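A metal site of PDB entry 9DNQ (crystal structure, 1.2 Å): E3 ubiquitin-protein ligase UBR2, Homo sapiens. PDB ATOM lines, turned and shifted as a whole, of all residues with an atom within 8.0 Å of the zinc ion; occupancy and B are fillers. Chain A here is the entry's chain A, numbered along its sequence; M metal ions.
N of Asp 22 lies close to SG of Cys 20. O of Cys 23 sits at hydrogen-bond distance from N of Lys 66 (2.8 Å). O of Ile 40 is in hydrogen-bond range of NE2 of His 44 (3.4 Å). The backbone carbonyl oxygen (O) of Arg 45 lies close to the side-chain sulfur (SG) of Cys 20 (3.7 Å). The side-chain hydroxyl of Ser 39 sits at hydrogen-bond distance from the backbone NH of His 41. The backbone carbonyl oxygen of Glu 67 sits close to a ring nitrogen (NE2) of His 41 (3.4 Å). A ring nitrogen (NE2) of His 41 is in hydrogen-bond range of the backbone carbonyl oxygen of Gly 68, 2.8 Å away.
Four residues have an atom within 4 Å of the zinc ion: Cys 20, Cys 23, His 41 and His 44.
The zinc ion is bound by ND1 of His 44 (2.0 Å), ND1 of His 41 (2.1 Å), SG of Cys 20 (2.3 Å) and SG of Cys 23 (2.3 Å). The zinc ion has four donor atoms within binding distance.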
ATOM      1  N   SER A  19       8.472  17.138  -1.403  1.00  0.00           N
ATOM      2  CA  SER A  19       9.305  18.300  -1.129  1.00  0.00           C
ATOM      3  C   SER A  19       8.469  19.547  -1.334  1.00  0.00           C
ATOM      4  O   SER A  19       7.757  19.673  -2.326  1.00  0.00           O
ATOM      5  CB  SER A  19      10.520  18.353  -2.058  1.00  0.00           C
ATOM      6  OG  SER A  19      11.390  19.411  -1.673  1.00  0.00           O
ATOM      7  N   CYS A  20       8.543  20.482  -0.388  1.00  0.00           N
ATOM      8  CA  CYS A  20       7.807  21.722  -0.515  1.00  0.00           C
ATOM      9  C   CYS A  20       8.621  22.707  -1.352  1.00  0.00           C
ATOM     10  O   CYS A  20       9.709  23.106  -0.957  1.00  0.00           O
ATOM     11  CB  CYS A  20       7.507  22.331   0.851  1.00  0.00           C
ATOM     12  SG  CYS A  20       6.501  23.799   0.637  1.00  0.00           S
ATOM     13  N   ARG A  21       8.084  23.102  -2.502  1.00  0.00           N
ATOM     14  CA  ARG A  21       8.808  24.055  -3.353  1.00  0.00           C
ATOM     15  C   ARG A  21       8.916  25.412  -2.680  1.00  0.00           C
ATOM     16  O   ARG A  21       9.895  26.137  -2.916  1.00  0.00           O
ATOM     17  CB  ARG A  21       8.125  24.197  -4.707  1.00  0.00           C
ATOM     18  CG  ARG A  21       8.004  22.906  -5.521  1.00  0.00           C
ATOM     19  CD  ARG A  21       6.947  23.060  -6.620  1.00  0.00           C
ATOM     20  NE  ARG A  21       6.688  21.815  -7.336  1.00  0.00           N
ATOM     21  CZ  ARG A  21       7.338  21.425  -8.419  1.00  0.00           C
ATOM     22  NH1 ARG A  21       8.275  22.178  -8.975  1.00  0.00           N
ATOM     23  NH2 ARG A  21       7.025  20.248  -8.964  1.00  0.00           N
ATOM     24  N   ASP A  22       7.939  25.768  -1.859  1.00  0.00           N
ATOM     25  CA  ASP A  22       7.950  27.063  -1.173  1.00  0.00           C
ATOM     26  C   ASP A  22       8.920  27.102   0.003  1.00  0.00           C
ATOM     27  O   ASP A  22       9.410  28.195   0.327  1.00  0.00           O
ATOM     28  CB  ASP A  22       6.547  27.411  -0.684  1.00  0.00           C
ATOM     29  CG  ASP A  22       5.610  27.719  -1.823  1.00  0.00           C
ATOM     30  OD1 ASP A  22       6.067  28.295  -2.829  1.00  0.00           O
ATOM     31  OD2 ASP A  22       4.428  27.370  -1.735  1.00  0.00           O
ATOM     32  N   CYS A  23       9.219  25.973   0.643  1.00  0.00           N
ATOM     33  CA  CYS A  23       9.952  25.986   1.899  1.00  0.00           C
ATOM     34  C   CYS A  23      11.267  25.215   1.911  1.00  0.00           C
ATOM     35  O   CYS A  23      12.131  25.526   2.732  1.00  0.00           O
ATOM     36  CB  CYS A  23       9.085  25.476   3.061  1.00  0.00           C
ATOM     37  SG  CYS A  23       7.550  26.368   3.329  1.00  0.00           S
ATOM     38  N   ALA A  24      11.421  24.198   1.071  1.00  0.00           N
ATOM     39  CA  ALA A  24      12.612  23.343   1.131  1.00  0.00           C
ATOM     40  C   ALA A  24      13.869  24.076   0.680  1.00  0.00           C
ATOM     41  O   ALA A  24      13.838  24.919  -0.226  1.00  0.00           O
ATOM     42  CB  ALA A  24      12.439  22.115   0.237  1.00  0.00           C
ATOM     43  N   LEU A  31       9.547  14.889   2.829  1.00  0.00           N
ATOM     44  CA  LEU A  31       8.755  14.295   3.890  1.00  0.00           C
ATOM     45  C   LEU A  31       8.079  13.036   3.372  1.00  0.00           C
ATOM     46  O   LEU A  31       7.692  12.954   2.193  1.00  0.00           O
ATOM     47  CB  LEU A  31       7.638  15.270   4.312  1.00  0.00           C
ATOM     48  CG  LEU A  31       8.134  16.600   4.889  1.00  0.00           C
ATOM     49  CD1 LEU A  31       6.939  17.512   5.164  1.00  0.00           C
ATOM     50  CD2 LEU A  31       8.910  16.397   6.164  1.00  0.00           C
ATOM     51  N   PHE A  36       3.916  14.696   5.561  1.00  0.00           N
ATOM     52  CA  PHE A  36       3.497  15.765   4.650  1.00  0.00           C
ATOM     53  C   PHE A  36       2.037  16.121   4.880  1.00  0.00           C
ATOM     54  O   PHE A  36       1.660  17.298   4.987  1.00  0.00           O
ATOM     55  CB  PHE A  36       3.713  15.306   3.200  1.00  0.00           C
ATOM     56  CG  PHE A  36       3.170  16.257   2.175  1.00  0.00           C
ATOM     57  CD1 PHE A  36       3.788  17.473   1.937  1.00  0.00           C
ATOM     58  CD2 PHE A  36       2.008  15.954   1.479  1.00  0.00           C
ATOM     59  CE1 PHE A  36       3.257  18.357   0.999  1.00  0.00           C
ATOM     60  CE2 PHE A  36       1.500  16.830   0.543  1.00  0.00           C
ATOM     61  CZ  PHE A  36       2.121  18.026   0.305  1.00  0.00           C
ATOM     62  N   SER A  39       1.231  18.275   7.806  1.00  0.00           N
ATOM     63  CA  SER A  39       2.121  19.429   7.881  1.00  0.00           C
ATOM     64  C   SER A  39       1.481  20.638   7.205  1.00  0.00           C
ATOM     65  O   SER A  39       0.547  20.511   6.422  1.00  0.00           O
ATOM     66  CB  SER A  39       3.463  19.120   7.208  1.00  0.00           C
ATOM     67  OG  SER A  39       3.385  19.322   5.802  1.00  0.00           O
ATOM     68  N   ILE A  40       2.050  21.819   7.480  1.00  0.00           N
ATOM     69  CA  ILE A  40       1.579  23.039   6.819  1.00  0.00           C
ATOM     70  C   ILE A  40       1.883  23.032   5.332  1.00  0.00           C
ATOM     71  O   ILE A  40       1.286  23.812   4.571  1.00  0.00           O
ATOM     72  CB  ILE A  40       2.136  24.327   7.449  1.00  0.00           C
ATOM     73  CG1 ILE A  40       3.657  24.402   7.293  1.00  0.00           C
ATOM     74  CG2 ILE A  40       1.722  24.440   8.910  1.00  0.00           C
ATOM     75  CD1 ILE A  40       4.239  25.758   7.669  1.00  0.00           C
ATOM     76  N   HIS A  41       2.797  22.184   4.877  1.00  0.00           N
ATOM     77  CA  HIS A  41       3.236  22.205   3.484  1.00  0.00           C
ATOM     78  C   HIS A  41       2.226  21.582   2.551  1.00  0.00           C
ATOM     79  O   HIS A  41       2.349  21.752   1.324  1.00  0.00           O
ATOM     80  CB  HIS A  41       4.609  21.549   3.356  1.00  0.00           C
ATOM     81  CG  HIS A  41       5.593  22.099   4.337  1.00  0.00           C
ATOM     82  ND1 HIS A  41       6.117  23.358   4.222  1.00  0.00           N
ATOM     83  CD2 HIS A  41       6.060  21.596   5.503  1.00  0.00           C
ATOM     84  CE1 HIS A  41       6.905  23.604   5.254  1.00  0.00           C
ATOM     85  NE2 HIS A  41       6.889  22.541   6.044  1.00  0.00           N
ATOM     86  N   ARG A  42       1.215  20.900   3.080  1.00  0.00           N
ATOM     87  CA  ARG A  42       0.202  20.299   2.223  1.00  0.00           C
ATOM     88  C   ARG A  42      -0.554  21.340   1.412  1.00  0.00           C
ATOM     89  O   ARG A  42      -1.118  21.009   0.368  1.00  0.00           O
ATOM     90  CB  ARG A  42      -0.722  19.412   3.055  1.00  0.00           C
ATOM     91  CG  ARG A  42      -1.724  20.158   3.892  1.00  0.00           C
ATOM     92  CD  ARG A  42      -2.765  19.211   4.462  1.00  0.00           C
ATOM     93  NE  ARG A  42      -3.612  18.645   3.413  1.00  0.00           N
ATOM     94  CZ  ARG A  42      -4.107  17.419   3.427  1.00  0.00           C
ATOM     95  NH1 ARG A  42      -3.826  16.567   4.402  1.00  0.00           N
ATOM     96  NH2 ARG A  42      -4.912  17.030   2.445  1.00  0.00           N
ATOM     97  N   ASP A  43      -0.574  22.596   1.863  1.00  0.00           N
ATOM     98  CA  ASP A  43      -1.232  23.702   1.170  1.00  0.00           C
ATOM     99  C   ASP A  43      -0.268  24.502   0.305  1.00  0.00           C
ATOM    100  O   ASP A  43      -0.709  25.464  -0.351  1.00  0.00           O
ATOM    101  CB  ASP A  43      -1.851  24.658   2.188  1.00  0.00           C
ATOM    102  CG  ASP A  43      -2.848  23.976   3.081  1.00  0.00           C
ATOM    103  OD1 ASP A  43      -2.721  24.138   4.310  1.00  0.00           O
ATOM    104  OD2 ASP A  43      -3.739  23.275   2.560  1.00  0.00           O
ATOM    105  N   HIS A  44       1.008  24.160   0.314  1.00  0.00           N
ATOM    106  CA  HIS A  44       1.999  24.926  -0.419  1.00  0.00           C
ATOM    107  C   HIS A  44       2.205  24.286  -1.786  1.00  0.00           C
ATOM    108  O   HIS A  44       1.655  23.227  -2.088  1.00  0.00           O
ATOM    109  CB  HIS A  44       3.311  24.947   0.376  1.00  0.00           C
ATOM    110  CG  HIS A  44       3.202  25.638   1.699  1.00  0.00           C
ATOM    111  ND1 HIS A  44       4.197  25.584   2.654  1.00  0.00           N
ATOM    112  CD2 HIS A  44       2.192  26.376   2.234  1.00  0.00           C
ATOM    113  CE1 HIS A  44       3.810  26.277   3.713  1.00  0.00           C
ATOM    114  NE2 HIS A  44       2.605  26.774   3.478  1.00  0.00           N
ATOM    115  N   ARG A  45       2.966  24.962  -2.644  1.00  0.00           N
ATOM    116  CA  ARG A  45       3.357  24.326  -3.884  1.00  0.00           C
ATOM    117  C   ARG A  45       4.391  23.257  -3.579  1.00  0.00           C
ATOM    118  O   ARG A  45       5.377  23.519  -2.871  1.00  0.00           O
ATOM    119  CB  ARG A  45       3.901  25.367  -4.850  1.00  0.00           C
ATOM    120  CG  ARG A  45       2.792  26.293  -5.341  1.00  0.00           C
ATOM    121  CD  ARG A  45       3.323  27.477  -6.095  1.00  0.00           C
ATOM    122  NE  ARG A  45       4.026  28.386  -5.194  1.00  0.00           N
ATOM    123  CZ  ARG A  45       4.390  29.620  -5.512  1.00  0.00           C
ATOM    124  NH1 ARG A  45       4.110  30.146  -6.693  1.00  0.00           N
ATOM    125  NH2 ARG A  45       5.046  30.352  -4.612  1.00  0.00           N
ATOM    126  N   TYR A  46       4.169  22.041  -4.073  1.00  0.00           N
ATOM    127  CA  TYR A  46       4.990  20.919  -3.643  1.00  0.00           C
ATOM    128  C   TYR A  46       5.323  20.026  -4.828  1.00  0.00           C
ATOM    129  O   TYR A  46       4.800  20.172  -5.934  1.00  0.00           O
ATOM    130  CB  TYR A  46       4.345  20.142  -2.489  1.00  0.00           C
ATOM    131  CG  TYR A  46       3.125  19.325  -2.863  1.00  0.00           C
ATOM    132  CD1 TYR A  46       3.251  18.021  -3.334  1.00  0.00           C
ATOM    133  CD2 TYR A  46       1.852  19.834  -2.668  1.00  0.00           C
ATOM    134  CE1 TYR A  46       2.145  17.248  -3.662  1.00  0.00           C
ATOM    135  CE2 TYR A  46       0.732  19.060  -2.979  1.00  0.00           C
ATOM    136  CZ  TYR A  46       0.893  17.770  -3.466  1.00  0.00           C
ATOM    137  OH  TYR A  46      -0.208  16.988  -3.784  1.00  0.00           O
ATOM    138  N   TRP A  65      13.776  23.267   6.148  1.00  0.00           N
ATOM    139  CA  TRP A  65      12.489  23.884   5.852  1.00  0.00           C
ATOM    140  C   TRP A  65      12.536  25.329   6.305  1.00  0.00           C
ATOM    141  O   TRP A  65      12.912  25.600   7.454  1.00  0.00           O
ATOM    142  CB  TRP A  65      11.378  23.124   6.613  1.00  0.00           C
ATOM    143  CG  TRP A  65      11.435  21.635   6.369  1.00  0.00           C
ATOM    144  CD1 TRP A  65      11.857  20.677   7.239  1.00  0.00           C
ATOM    145  CD2 TRP A  65      11.117  20.957   5.149  1.00  0.00           C
ATOM    146  NE1 TRP A  65      11.806  19.439   6.652  1.00  0.00           N
ATOM    147  CE2 TRP A  65      11.349  19.579   5.367  1.00  0.00           C
ATOM    148  CE3 TRP A  65      10.647  21.378   3.903  1.00  0.00           C
ATOM    149  CZ2 TRP A  65      11.136  18.626   4.372  1.00  0.00           C
ATOM    150  CZ3 TRP A  65      10.418  20.433   2.926  1.00  0.00           C
ATOM    151  CH2 TRP A  65      10.670  19.068   3.167  1.00  0.00           C
ATOM    152  N   LYS A  66      12.189  26.266   5.428  1.00  0.00           N
ATOM    153  CA  LYS A  66      12.286  27.666   5.831  1.00  0.00           C
ATOM    154  C   LYS A  66      11.286  27.985   6.946  1.00  0.00           C
ATOM    155  O   LYS A  66      11.534  28.898   7.756  1.00  0.00           O
ATOM    156  CB  LYS A  66      12.108  28.597   4.632  1.00  0.00           C
ATOM    157  CG  LYS A  66      10.682  28.995   4.313  1.00  0.00           C
ATOM    158  CD  LYS A  66      10.603  29.763   2.997  1.00  0.00           C
ATOM    159  CE  LYS A  66       9.202  30.338   2.784  1.00  0.00           C
ATOM    160  NZ  LYS A  66       8.927  30.617   1.347  1.00  0.00           N
ATOM    161  N   GLU A  67      10.196  27.224   7.014  1.00  0.00           N
ATOM    162  CA  GLU A  67       9.196  27.310   8.070  1.00  0.00           C
ATOM    163  C   GLU A  67       8.537  25.935   8.174  1.00  0.00           C
ATOM    164  O   GLU A  67       8.683  25.097   7.281  1.00  0.00           O
ATOM    165  CB  GLU A  67       8.146  28.367   7.752  1.00  0.00           C
ATOM    166  CG  GLU A  67       7.302  28.000   6.557  1.00  0.00           C
ATOM    167  CD  GLU A  67       6.340  29.097   6.198  1.00  0.00           C
ATOM    168  OE1 GLU A  67       6.711  29.959   5.371  1.00  0.00           O
ATOM    169  OE2 GLU A  67       5.206  29.096   6.741  1.00  0.00           O
ATOM    170  N   GLY A  68       7.836  25.715   9.289  1.00  0.00           N
ATOM    171  CA  GLY A  68       7.102  24.495   9.511  1.00  0.00           C
ATOM    172  C   GLY A  68       7.923  23.212   9.518  1.00  0.00           C
ATOM    173  O   GLY A  68       7.684  22.291   8.728  1.00  0.00           O
HETATM  174 ZN    ZN M   1       6.061  24.747   2.657  1.00  0.00          ZN
